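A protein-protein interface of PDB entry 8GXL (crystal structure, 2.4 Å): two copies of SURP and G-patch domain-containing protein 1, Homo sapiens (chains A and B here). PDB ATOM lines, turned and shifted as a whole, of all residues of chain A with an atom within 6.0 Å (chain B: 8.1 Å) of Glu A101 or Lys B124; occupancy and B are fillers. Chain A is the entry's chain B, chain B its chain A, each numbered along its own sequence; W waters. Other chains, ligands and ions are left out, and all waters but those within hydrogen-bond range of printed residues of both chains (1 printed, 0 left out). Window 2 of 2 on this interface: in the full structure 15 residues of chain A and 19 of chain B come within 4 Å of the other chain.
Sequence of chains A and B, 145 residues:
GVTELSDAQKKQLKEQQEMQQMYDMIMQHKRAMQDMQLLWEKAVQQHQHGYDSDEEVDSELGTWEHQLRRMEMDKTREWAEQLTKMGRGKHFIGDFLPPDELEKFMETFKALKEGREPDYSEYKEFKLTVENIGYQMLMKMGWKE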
ATOM      1  N   LEU A  97     -10.570   7.473  -1.503  1.00  0.00           N
ATOM      2  CA  LEU A  97     -11.067   8.763  -1.049  1.00  0.00           C
ATOM      3  C   LEU A  97      -9.927   9.723  -0.722  1.00  0.00           C
ATOM      4  O   LEU A  97      -8.930   9.324  -0.106  1.00  0.00           O
ATOM      5  CB  LEU A  97     -11.962   8.606   0.195  1.00  0.00           C
ATOM      6  CG  LEU A  97     -13.316   7.926   0.006  1.00  0.00           C
ATOM      7  CD1 LEU A  97     -14.051   7.855   1.333  1.00  0.00           C
ATOM      8  CD2 LEU A  97     -14.142   8.672  -1.042  1.00  0.00           C
ATOM      9  N   PRO A  98     -10.047  10.989  -1.112  1.00  0.00           N
ATOM     10  CA  PRO A  98      -9.079  12.000  -0.677  1.00  0.00           C
ATOM     11  C   PRO A  98      -9.248  12.294   0.800  1.00  0.00           C
ATOM     12  O   PRO A  98     -10.323  12.036   1.366  1.00  0.00           O
ATOM     13  CB  PRO A  98      -9.438  13.221  -1.536  1.00  0.00           C
ATOM     14  CG  PRO A  98     -10.893  13.043  -1.821  1.00  0.00           C
ATOM     15  CD  PRO A  98     -11.080  11.558  -1.994  1.00  0.00           C
ATOM     16  N   PRO A  99      -8.212  12.872   1.450  1.00  0.00           N
ATOM     17  CA  PRO A  99      -8.175  12.957   2.919  1.00  0.00           C
ATOM     18  C   PRO A  99      -9.461  13.389   3.601  1.00  0.00           C
ATOM     19  O   PRO A  99      -9.919  12.722   4.536  1.00  0.00           O
ATOM     20  CB  PRO A  99      -7.069  13.989   3.163  1.00  0.00           C
ATOM     21  CG  PRO A  99      -6.127  13.774   2.027  1.00  0.00           C
ATOM     22  CD  PRO A  99      -6.983  13.417   0.841  1.00  0.00           C
ATOM     23  N   ASP A 100     -10.044  14.505   3.162  1.00  0.00           N
ATOM     24  CA  ASP A 100     -11.227  15.019   3.846  1.00  0.00           C
ATOM     25  C   ASP A 100     -12.408  14.058   3.723  1.00  0.00           C
ATOM     26  O   ASP A 100     -13.142  13.836   4.696  1.00  0.00           O
ATOM     27  CB  ASP A 100     -11.587  16.402   3.309  1.00  0.00           C
ATOM     28  CG  ASP A 100     -10.715  17.507   3.908  1.00  0.00           C
ATOM     29  OD1 ASP A 100      -9.802  17.190   4.711  1.00  0.00           O
ATOM     30  OD2 ASP A 100     -10.950  18.693   3.576  1.00  0.00           O
ATOM     31  N   GLU A 101     -12.603  13.465   2.543  1.00  0.00           N
ATOM     32  CA  GLU A 101     -13.695  12.512   2.397  1.00  0.00           C
ATOM     33  C   GLU A 101     -13.464  11.273   3.257  1.00  0.00           C
ATOM     34  O   GLU A 101     -14.418  10.711   3.803  1.00  0.00           O
ATOM     35  CB  GLU A 101     -13.881  12.122   0.931  1.00  0.00           C
ATOM     36  CG  GLU A 101     -14.888  12.960   0.185  1.00  0.00           C
ATOM     37  CD  GLU A 101     -14.301  14.286  -0.235  1.00  0.00           C
ATOM     38  OE1 GLU A 101     -13.060  14.441  -0.111  1.00  0.00           O
ATOM     39  OE2 GLU A 101     -15.077  15.166  -0.691  1.00  0.00           O
ATOM     40  N   LEU A 102     -12.208  10.839   3.399  1.00  0.00           N
ATOM     41  CA  LEU A 102     -11.924   9.655   4.209  1.00  0.00           C
ATOM     42  C   LEU A 102     -12.308   9.877   5.669  1.00  0.00           C
ATOM     43  O   LEU A 102     -12.962   9.027   6.285  1.00  0.00           O
ATOM     44  CB  LEU A 102     -10.446   9.281   4.091  1.00  0.00           C
ATOM     45  CG  LEU A 102      -9.992   7.917   4.624  1.00  0.00           C
ATOM     46  CD1 LEU A 102     -10.986   6.816   4.291  1.00  0.00           C
ATOM     47  CD2 LEU A 102      -8.641   7.576   4.042  1.00  0.00           C
ATOM     48  N   GLU A 103     -11.902  11.014   6.245  1.00  0.00           N
ATOM     49  CA  GLU A 103     -12.221  11.274   7.648  1.00  0.00           C
ATOM     50  C   GLU A 103     -13.728  11.268   7.867  1.00  0.00           C
ATOM     51  O   GLU A 103     -14.225  10.642   8.812  1.00  0.00           O
ATOM     52  CB  GLU A 103     -11.604  12.603   8.100  1.00  0.00           C
ATOM     53  CG  GLU A 103     -10.368  12.461   9.003  1.00  0.00           C
ATOM     54  CD  GLU A 103      -9.809  13.809   9.501  1.00  0.00           C
ATOM     55  OE1 GLU A 103      -9.963  14.832   8.793  1.00  0.00           O
ATOM     56  OE2 GLU A 103      -9.201  13.838  10.600  1.00  0.00           O
ATOM     57  N   LYS A 104     -14.475  11.933   6.980  1.00  0.00           N
ATOM     58  CA  LYS A 104     -15.927  11.962   7.116  1.00  0.00           C
ATOM     59  C   LYS A 104     -16.529  10.564   6.961  1.00  0.00           C
ATOM     60  O   LYS A 104     -17.379  10.156   7.762  1.00  0.00           O
ATOM     61  CB  LYS A 104     -16.518  12.933   6.098  1.00  0.00           C
ATOM     62  CG  LYS A 104     -17.990  13.186   6.301  1.00  0.00           C
ATOM     63  CD  LYS A 104     -18.254  13.899   7.609  1.00  0.00           C
ATOM     64  CE  LYS A 104     -17.604  15.277   7.642  1.00  0.00           C
ATOM     65  NZ  LYS A 104     -18.523  16.283   8.271  1.00  0.00           N
ATOM     66  N   PHE A 105     -16.085   9.824   5.942  1.00  0.00           N
ATOM     67  CA  PHE A 105     -16.518   8.447   5.714  1.00  0.00           C
ATOM     68  C   PHE A 105     -16.329   7.587   6.961  1.00  0.00           C
ATOM     69  O   PHE A 105     -17.243   6.863   7.377  1.00  0.00           O
ATOM     70  CB  PHE A 105     -15.738   7.861   4.524  1.00  0.00           C
ATOM     71  CG  PHE A 105     -16.102   6.431   4.185  1.00  0.00           C
ATOM     72  CD1 PHE A 105     -17.083   6.156   3.225  1.00  0.00           C
ATOM     73  CD2 PHE A 105     -15.457   5.361   4.807  1.00  0.00           C
ATOM     74  CE1 PHE A 105     -17.422   4.847   2.902  1.00  0.00           C
ATOM     75  CE2 PHE A 105     -15.791   4.047   4.493  1.00  0.00           C
ATOM     76  CZ  PHE A 105     -16.775   3.791   3.534  1.00  0.00           C
ATOM     77  N   MET A 106     -15.128   7.643   7.554  1.00  0.00           N
ATOM     78  CA  MET A 106     -14.812   6.819   8.719  1.00  0.00           C
ATOM     79  C   MET A 106     -15.631   7.246   9.935  1.00  0.00           C
ATOM     80  O   MET A 106     -16.106   6.396  10.702  1.00  0.00           O
ATOM     81  CB  MET A 106     -13.315   6.899   9.021  1.00  0.00           C
ATOM     82  CG  MET A 106     -12.451   6.082   8.063  1.00  0.00           C
ATOM     83  SD  MET A 106     -12.947   4.345   7.971  1.00  0.00           S
ATOM     84  CE  MET A 106     -12.232   3.841   6.420  1.00  0.00           C
ATOM     85  N   GLU A 125     -24.727  10.722   1.962  1.00  0.00           N
ATOM     86  CA  GLU A 125     -23.422  10.824   1.327  1.00  0.00           C
ATOM     87  C   GLU A 125     -22.625   9.546   1.537  1.00  0.00           C
ATOM     88  O   GLU A 125     -22.042   9.016   0.589  1.00  0.00           O
ATOM     89  CB  GLU A 125     -22.667  12.043   1.858  1.00  0.00           C
ATOM     90  CG  GLU A 125     -21.176  12.075   1.487  1.00  0.00           C
ATOM     91  CD  GLU A 125     -20.519  13.434   1.745  1.00  0.00           C
ATOM     92  OE1 GLU A 125     -19.268  13.523   1.682  1.00  0.00           O
ATOM     93  OE2 GLU A 125     -21.259  14.409   2.002  1.00  0.00           O
ATOM     94  N   LEU A 128     -24.071   6.646  -0.645  1.00  0.00           N
ATOM     95  CA  LEU A 128     -23.700   6.755  -2.049  1.00  0.00           C
ATOM     96  C   LEU A 128     -22.231   6.428  -2.234  1.00  0.00           C
ATOM     97  O   LEU A 128     -21.839   5.810  -3.232  1.00  0.00           O
ATOM     98  CB  LEU A 128     -24.005   8.159  -2.560  1.00  0.00           C
ATOM     99  CG  LEU A 128     -25.476   8.431  -2.916  1.00  0.00           C
ATOM    100  CD1 LEU A 128     -25.721   9.938  -3.028  1.00  0.00           C
ATOM    101  CD2 LEU A 128     -25.851   7.729  -4.223  1.00  0.00           C
ATOM    102  N   GLN B  37      -9.545  17.573  -8.330  1.00  0.00           N
ATOM    103  CA  GLN B  37      -9.334  17.385  -6.897  1.00  0.00           C
ATOM    104  C   GLN B  37      -7.925  17.803  -6.493  1.00  0.00           C
ATOM    105  O   GLN B  37      -7.731  18.490  -5.485  1.00  0.00           O
ATOM    106  CB  GLN B  37      -9.586  15.923  -6.531  1.00  0.00           C
ATOM    107  CG  GLN B  37      -9.201  15.554  -5.112  1.00  0.00           C
ATOM    108  CD  GLN B  37     -10.019  16.306  -4.072  1.00  0.00           C
ATOM    109  OE1 GLN B  37     -11.184  16.632  -4.304  1.00  0.00           O
ATOM    110  NE2 GLN B  37      -9.409  16.587  -2.920  1.00  0.00           N
ATOM    111  N   TRP B  40      -7.582  21.540  -6.768  1.00  0.00           N
ATOM    112  CA  TRP B  40      -8.313  22.187  -5.691  1.00  0.00           C
ATOM    113  C   TRP B  40      -7.570  22.056  -4.364  1.00  0.00           C
ATOM    114  O   TRP B  40      -7.533  23.006  -3.577  1.00  0.00           O
ATOM    115  CB  TRP B  40      -9.712  21.602  -5.593  1.00  0.00           C
ATOM    116  CG  TRP B  40     -10.467  22.108  -4.437  1.00  0.00           C
ATOM    117  CD1 TRP B  40     -11.285  23.205  -4.398  1.00  0.00           C
ATOM    118  CD2 TRP B  40     -10.480  21.546  -3.122  1.00  0.00           C
ATOM    119  NE1 TRP B  40     -11.813  23.349  -3.136  1.00  0.00           N
ATOM    120  CE2 TRP B  40     -11.330  22.342  -2.336  1.00  0.00           C
ATOM    121  CE3 TRP B  40      -9.856  20.439  -2.536  1.00  0.00           C
ATOM    122  CZ2 TRP B  40     -11.572  22.064  -0.996  1.00  0.00           C
ATOM    123  CZ3 TRP B  40     -10.095  20.170  -1.203  1.00  0.00           C
ATOM    124  CH2 TRP B  40     -10.944  20.976  -0.451  1.00  0.00           C
ATOM    125  N   GLU B  41      -6.960  20.896  -4.110  1.00  0.00           N
ATOM    126  CA  GLU B  41      -6.220  20.704  -2.871  1.00  0.00           C
ATOM    127  C   GLU B  41      -5.082  21.707  -2.750  1.00  0.00           C
ATOM    128  O   GLU B  41      -4.807  22.221  -1.658  1.00  0.00           O
ATOM    129  CB  GLU B  41      -5.691  19.275  -2.795  1.00  0.00           C
ATOM    130  CG  GLU B  41      -6.782  18.296  -2.402  1.00  0.00           C
ATOM    131  CD  GLU B  41      -6.326  16.845  -2.363  1.00  0.00           C
ATOM    132  OE1 GLU B  41      -5.102  16.599  -2.309  1.00  0.00           O
ATOM    133  OE2 GLU B  41      -7.203  15.946  -2.389  1.00  0.00           O
ATOM    134  N   ARG B  69     -13.689  24.661  -7.792  1.00  0.00           N
ATOM    135  CA  ARG B  69     -14.897  23.933  -7.414  1.00  0.00           C
ATOM    136  C   ARG B  69     -16.006  24.134  -8.433  1.00  0.00           C
ATOM    137  O   ARG B  69     -16.760  23.199  -8.724  1.00  0.00           O
ATOM    138  CB  ARG B  69     -15.387  24.377  -6.036  1.00  0.00           C
ATOM    139  CG  ARG B  69     -14.756  23.636  -4.871  1.00  0.00           C
ATOM    140  CD  ARG B  69     -15.130  22.157  -4.854  1.00  0.00           C
ATOM    141  NE  ARG B  69     -14.120  21.350  -4.169  1.00  0.00           N
ATOM    142  CZ  ARG B  69     -13.962  20.042  -4.345  1.00  0.00           C
ATOM    143  NH1 ARG B  69     -14.754  19.386  -5.186  1.00  0.00           N
ATOM    144  NH2 ARG B  69     -13.012  19.384  -3.687  1.00  0.00           N
ATOM    145  N   GLU B  72     -15.397  22.159 -11.494  1.00  0.00           N
ATOM    146  CA  GLU B  72     -15.626  20.744 -11.249  1.00  0.00           C
ATOM    147  C   GLU B  72     -17.102  20.412 -11.374  1.00  0.00           C
ATOM    148  O   GLU B  72     -17.463  19.414 -12.006  1.00  0.00           O
ATOM    149  CB  GLU B  72     -15.105  20.322  -9.880  1.00  0.00           C
ATOM    150  CG  GLU B  72     -15.256  18.815  -9.711  1.00  0.00           C
ATOM    151  CD  GLU B  72     -15.279  18.349  -8.275  1.00  0.00           C
ATOM    152  OE1 GLU B  72     -14.234  18.456  -7.589  1.00  0.00           O
ATOM    153  OE2 GLU B  72     -16.330  17.839  -7.841  1.00  0.00           O
ATOM    154  N   MET B  73     -17.967  21.240 -10.780  1.00  0.00           N
ATOM    155  CA  MET B  73     -19.403  21.043 -10.929  1.00  0.00           C
ATOM    156  C   MET B  73     -19.801  21.045 -12.398  1.00  0.00           C
ATOM    157  O   MET B  73     -20.642  20.243 -12.821  1.00  0.00           O
ATOM    158  CB  MET B  73     -20.173  22.123 -10.171  1.00  0.00           C
ATOM    159  CG  MET B  73     -20.046  22.048  -8.654  1.00  0.00           C
ATOM    160  SD  MET B  73     -20.999  23.354  -7.820  1.00  0.00           S
ATOM    161  CE  MET B  73     -20.452  23.123  -6.119  1.00  0.00           C
ATOM    162  N   THR B  76     -18.911  17.730 -13.858  1.00  0.00           N
ATOM    163  CA  THR B  76     -19.949  16.786 -13.462  1.00  0.00           C
ATOM    164  C   THR B  76     -21.201  16.966 -14.308  1.00  0.00           C
ATOM    165  O   THR B  76     -21.792  15.982 -14.779  1.00  0.00           O
ATOM    166  CB  THR B  76     -20.275  16.964 -11.978  1.00  0.00           C
ATOM    167  OG1 THR B  76     -19.084  16.782 -11.224  1.00  0.00           O
ATOM    168  CG2 THR B  76     -21.288  15.941 -11.509  1.00  0.00           C
ATOM    169  N   THR B 108     -31.246  19.514  -9.036  1.00  0.00           N
ATOM    170  CA  THR B 108     -29.825  19.845  -8.985  1.00  0.00           C
ATOM    171  C   THR B 108     -29.243  19.945 -10.390  1.00  0.00           C
ATOM    172  O   THR B 108     -28.504  20.890 -10.700  1.00  0.00           O
ATOM    173  CB  THR B 108     -29.068  18.806  -8.164  1.00  0.00           C
ATOM    174  OG1 THR B 108     -29.643  18.727  -6.861  1.00  0.00           O
ATOM    175  CG2 THR B 108     -27.605  19.201  -8.032  1.00  0.00           C
ATOM    176  N   PRO B 118     -25.705  24.898  -6.415  1.00  0.00           N
ATOM    177  CA  PRO B 118     -26.498  24.246  -5.367  1.00  0.00           C
ATOM    178  C   PRO B 118     -25.754  24.219  -4.042  1.00  0.00           C
ATOM    179  O   PRO B 118     -24.555  24.498  -3.962  1.00  0.00           O
ATOM    180  CB  PRO B 118     -26.707  22.828  -5.919  1.00  0.00           C
ATOM    181  CG  PRO B 118     -25.573  22.617  -6.840  1.00  0.00           C
ATOM    182  CD  PRO B 118     -25.264  23.955  -7.455  1.00  0.00           C
ATOM    183  N   ASP B 119     -26.510  23.907  -2.982  1.00  0.00           N
ATOM    184  CA  ASP B 119     -25.932  23.406  -1.736  1.00  0.00           C
ATOM    185  C   ASP B 119     -24.821  22.427  -2.050  1.00  0.00           C
ATOM    186  O   ASP B 119     -24.981  21.555  -2.908  1.00  0.00           O
ATOM    187  CB  ASP B 119     -26.994  22.671  -0.912  1.00  0.00           C
ATOM    188  CG  ASP B 119     -27.559  23.506   0.203  1.00  0.00           C
ATOM    189  OD1 ASP B 119     -27.176  24.693   0.318  1.00  0.00           O
ATOM    190  OD2 ASP B 119     -28.396  22.962   0.962  1.00  0.00           O
ATOM    191  N   TYR B 120     -23.693  22.555  -1.353  1.00  0.00           N
ATOM    192  CA  TYR B 120     -22.597  21.653  -1.662  1.00  0.00           C
ATOM    193  C   TYR B 120     -22.942  20.217  -1.274  1.00  0.00           C
ATOM    194  O   TYR B 120     -22.440  19.271  -1.895  1.00  0.00           O
ATOM    195  CB  TYR B 120     -21.303  22.098  -0.981  1.00  0.00           C
ATOM    196  CG  TYR B 120     -20.090  21.371  -1.526  1.00  0.00           C
ATOM    197  CD1 TYR B 120     -19.610  21.635  -2.813  1.00  0.00           C
ATOM    198  CD2 TYR B 120     -19.438  20.400  -0.767  1.00  0.00           C
ATOM    199  CE1 TYR B 120     -18.493  20.953  -3.324  1.00  0.00           C
ATOM    200  CE2 TYR B 120     -18.326  19.713  -1.264  1.00  0.00           C
ATOM    201  CZ  TYR B 120     -17.861  19.994  -2.541  1.00  0.00           C
ATOM    202  OH  TYR B 120     -16.769  19.310  -3.014  1.00  0.00           O
ATOM    203  N   SER B 121     -23.801  20.028  -0.271  1.00  0.00           N
ATOM    204  CA  SER B 121     -24.185  18.663   0.042  1.00  0.00           C
ATOM    205  C   SER B 121     -25.203  18.162  -0.968  1.00  0.00           C
ATOM    206  O   SER B 121     -25.278  16.957  -1.233  1.00  0.00           O
ATOM    207  CB  SER B 121     -24.703  18.566   1.480  1.00  0.00           C
ATOM    208  OG  SER B 121     -26.086  18.823   1.570  1.00  0.00           O
ATOM    209  N   GLU B 122     -25.945  19.084  -1.566  1.00  0.00           N
ATOM    210  CA  GLU B 122     -26.829  18.757  -2.673  1.00  0.00           C
ATOM    211  C   GLU B 122     -26.020  18.422  -3.917  1.00  0.00           C
ATOM    212  O   GLU B 122     -26.367  17.504  -4.669  1.00  0.00           O
ATOM    213  CB  GLU B 122     -27.762  19.944  -2.917  1.00  0.00           C
ATOM    214  CG  GLU B 122     -28.957  19.732  -3.783  1.00  0.00           C
ATOM    215  CD  GLU B 122     -29.862  20.983  -3.842  1.00  0.00           C
ATOM    216  OE1 GLU B 122     -30.209  21.535  -2.760  1.00  0.00           O
ATOM    217  OE2 GLU B 122     -30.207  21.417  -4.975  1.00  0.00           O
ATOM    218  N   TYR B 123     -24.917  19.138  -4.130  1.00  0.00           N
ATOM    219  CA  TYR B 123     -24.067  18.833  -5.272  1.00  0.00           C
ATOM    220  C   TYR B 123     -23.318  17.515  -5.080  1.00  0.00           C
ATOM    221  O   TYR B 123     -23.216  16.719  -6.017  1.00  0.00           O
ATOM    222  CB  TYR B 123     -23.076  19.965  -5.532  1.00  0.00           C
ATOM    223  CG  TYR B 123     -21.960  19.504  -6.425  1.00  0.00           C
ATOM    224  CD1 TYR B 123     -22.192  19.284  -7.769  1.00  0.00           C
ATOM    225  CD2 TYR B 123     -20.687  19.234  -5.919  1.00  0.00           C
ATOM    226  CE1 TYR B 123     -21.200  18.834  -8.602  1.00  0.00           C
ATOM    227  CE2 TYR B 123     -19.674  18.768  -6.758  1.00  0.00           C
ATOM    228  CZ  TYR B 123     -19.949  18.575  -8.106  1.00  0.00           C
ATOM    229  OH  TYR B 123     -18.992  18.125  -8.977  1.00  0.00           O
ATOM    230  N   LYS B 124     -22.764  17.268  -3.889  1.00  0.00           N
ATOM    231  CA  LYS B 124     -21.992  16.048  -3.725  1.00  0.00           C
ATOM    232  C   LYS B 124     -22.854  14.822  -3.983  1.00  0.00           C
ATOM    233  O   LYS B 124     -22.401  13.843  -4.584  1.00  0.00           O
ATOM    234  CB  LYS B 124     -21.355  15.972  -2.341  1.00  0.00           C
ATOM    235  CG  LYS B 124     -20.136  15.010  -2.376  1.00  0.00           C
ATOM    236  CD  LYS B 124     -19.414  14.878  -1.034  1.00  0.00           C
ATOM    237  CE  LYS B 124     -18.747  16.202  -0.598  1.00  0.00           C
ATOM    238  NZ  LYS B 124     -19.527  16.870   0.490  1.00  0.00           N
ATOM    239  N   GLU B 125     -24.106  14.876  -3.578  1.00  0.00           N
ATOM    240  CA  GLU B 125     -24.939  13.703  -3.726  1.00  0.00           C
ATOM    241  C   GLU B 125     -25.371  13.519  -5.178  1.00  0.00           C
ATOM    242  O   GLU B 125     -25.490  12.379  -5.655  1.00  0.00           O
ATOM    243  CB  GLU B 125     -26.078  13.821  -2.710  1.00  0.00           C
ATOM    244  CG  GLU B 125     -27.450  13.397  -3.086  1.00  0.00           C
ATOM    245  CD  GLU B 125     -28.423  13.816  -1.984  1.00  0.00           C
ATOM    246  OE1 GLU B 125     -27.960  14.009  -0.829  1.00  0.00           O
ATOM    247  OE2 GLU B 125     -29.635  13.911  -2.254  1.00  0.00           O
ATOM    248  N   PHE B 126     -25.529  14.619  -5.912  1.00  0.00           N
ATOM    249  CA  PHE B 126     -25.755  14.529  -7.348  1.00  0.00           C
ATOM    250  C   PHE B 126     -24.530  13.953  -8.064  1.00  0.00           C
ATOM    251  O   PHE B 126     -24.654  13.049  -8.905  1.00  0.00           O
ATOM    252  CB  PHE B 126     -26.118  15.910  -7.881  1.00  0.00           C
ATOM    253  CG  PHE B 126     -26.158  16.005  -9.374  1.00  0.00           C
ATOM    254  CD1 PHE B 126     -27.311  15.691 -10.067  1.00  0.00           C
ATOM    255  CD2 PHE B 126     -25.056  16.455 -10.084  1.00  0.00           C
ATOM    256  CE1 PHE B 126     -27.367  15.817 -11.450  1.00  0.00           C
ATOM    257  CE2 PHE B 126     -25.099  16.576 -11.454  1.00  0.00           C
ATOM    258  CZ  PHE B 126     -26.248  16.262 -12.141  1.00  0.00           C
ATOM    259  N   LYS B 127     -23.345  14.459  -7.721  1.00  0.00           N
ATOM    260  CA  LYS B 127     -22.104  13.934  -8.275  1.00  0.00           C
ATOM    261  C   LYS B 127     -21.988  12.429  -8.062  1.00  0.00           C
ATOM    262  O   LYS B 127     -21.664  11.683  -8.998  1.00  0.00           O
ATOM    263  CB  LYS B 127     -20.921  14.646  -7.630  1.00  0.00           C
ATOM    264  CG  LYS B 127     -19.633  14.409  -8.333  1.00  0.00           C
ATOM    265  CD  LYS B 127     -18.465  15.003  -7.561  1.00  0.00           C
ATOM    266  CE  LYS B 127     -17.373  13.987  -7.324  1.00  0.00           C
ATOM    267  NZ  LYS B 127     -16.056  14.667  -7.197  1.00  0.00           N
ATOM    268  N   LEU B 128     -22.210  11.962  -6.828  1.00  0.00           N
ATOM    269  CA  LEU B 128     -22.045  10.538  -6.572  1.00  0.00           C
ATOM    270  C   LEU B 128     -23.117   9.748  -7.297  1.00  0.00           C
ATOM    271  O   LEU B 128     -22.847   8.666  -7.831  1.00  0.00           O
ATOM    272  CB  LEU B 128     -22.067  10.263  -5.070  1.00  0.00           C
ATOM    273  CG  LEU B 128     -20.847  10.747  -4.251  1.00  0.00           C
ATOM    274  CD1 LEU B 128     -21.133  10.771  -2.751  1.00  0.00           C
ATOM    275  CD2 LEU B 128     -19.603   9.901  -4.514  1.00  0.00           C
ATOM    276  N   THR B 129     -24.333  10.293  -7.354  1.00  0.00           N
ATOM    277  CA  THR B 129     -25.421   9.596  -8.022  1.00  0.00           C
ATOM    278  C   THR B 129     -25.130   9.477  -9.505  1.00  0.00           C
ATOM    279  O   THR B 129     -25.323   8.409 -10.098  1.00  0.00           O
ATOM    280  CB  THR B 129     -26.740  10.331  -7.793  1.00  0.00           C
ATOM    281  OG1 THR B 129     -27.000  10.430  -6.385  1.00  0.00           O
ATOM    282  CG2 THR B 129     -27.898   9.608  -8.484  1.00  0.00           C
ATOM    283  N   VAL B 130     -24.638  10.562 -10.108  1.00  0.00           N
ATOM    284  CA  VAL B 130     -24.308  10.529 -11.520  1.00  0.00           C
ATOM    285  C   VAL B 130     -23.284   9.437 -11.767  1.00  0.00           C
ATOM    286  O   VAL B 130     -23.415   8.621 -12.689  1.00  0.00           O
ATOM    287  CB  VAL B 130     -23.797  11.910 -11.984  1.00  0.00           C
ATOM    288  CG1 VAL B 130     -23.229  11.817 -13.391  1.00  0.00           C
ATOM    289  CG2 VAL B 130     -24.915  12.923 -11.930  1.00  0.00           C
ATOM    290  N   GLU B 131     -22.268   9.380 -10.908  1.00  0.00           N
ATOM    291  CA  GLU B 131     -21.209   8.404 -11.091  1.00  0.00           C
ATOM    292  C   GLU B 131     -21.727   6.986 -10.937  1.00  0.00           C
ATOM    293  O   GLU B 131     -21.347   6.099 -11.709  1.00  0.00           O
ATOM    294  CB  GLU B 131     -20.093   8.661 -10.097  1.00  0.00           C
ATOM    295  CG  GLU B 131     -19.361   9.918 -10.396  1.00  0.00           C
ATOM    296  CD  GLU B 131     -18.021   9.882  -9.777  1.00  0.00           C
ATOM    297  OE1 GLU B 131     -17.156   9.159 -10.342  1.00  0.00           O
ATOM    298  OE2 GLU B 131     -17.858  10.523  -8.708  1.00  0.00           O
HETATM  299  O   HOH W   1     -11.322  16.972  -0.289  1.00  0.00           O
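Glu A101 touches just one residue of chain B: Lys B124. Of the printed residues of chain B, Leu A128 touches Glu B125 (3.6 Å), Leu B128 (3.8 Å) and Thr B129 (3.6 Å). Arg B69 touches none of the printed residues of chain A. Of chain A, only Glu A101 (3.8 Å) and Glu A125 (3.0 Å) come within 4 Å of Lys B124. Printed residues of chain A within 4 Å of Leu B128: Glu A125 (3.9 Å) and Leu A128 (3.8 Å).
The side-chain amino group (NZ) of Lys B124 is in salt-bridge range of the side-chain carboxylate (OE2) of Glu A125 (3.4 Å).
Glu A125 touches Leu B128, and with the chains exchanged Leu A128 touches Glu B125. Leu B128 touches its own counterpart, Leu A128. Positions printed for both chains: 125 and 128. Of the 8 pairs that touch across the chains among the printed residues, 3 have their exchanged pair printed and touching as well.
Pro A98 touches Gln B37 (CB to NE2, 3.6 Å). Pro A98 touches Glu B41 (CB to OE2, 3.6 Å). Glu A101 touches Lys B124 (OE2 to CE, 3.8 Å). Glu A125 touches Leu B128. Leu A128 touches Glu B125 (CD1 to O, 3.6 Å). CB of Leu A128 touches CB of Leu B128 (3.8 Å). Thr B129 touches Leu A128.
Water W1 lies within hydrogen-bond range of the side-chain carboxylate of Glu A101 (3.1 Å) and the side-chain amide nitrogen of Gln B37 (3.3 Å).
The side-chain amide oxygen (OE1) of Gln B37 sits at hydrogen-bond distance from the guanidinium group (NH2) of Arg B69, 3.4 Å away. O of Glu B125 sits at hydrogen-bond distance from OG1 of Thr B129 (2.6 Å).
Printed residues of chain B that touch a printed residue of chain A: Gln B37, Glu B41, Lys B124, Glu B125, Leu B128 and Thr B129. Of the 12 printed residues of chain A, 4 touch a printed residue of chain B. Printed residues of chain A that touch a printed residue of chain B: Pro A98, Glu A101, Glu A125 and Leu A128. Hydrophobic or aromatic side chains of chain A that line the printed part of chain B: Pro A98 and Leu A128. Among the printed residues, 8 pairs touch across the chains. Among the printed residues, Asp or Glu carboxylates within 4 Å of a Lys or Arg side-chain nitrogen of the other chain: Glu A125 with Lys B124.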
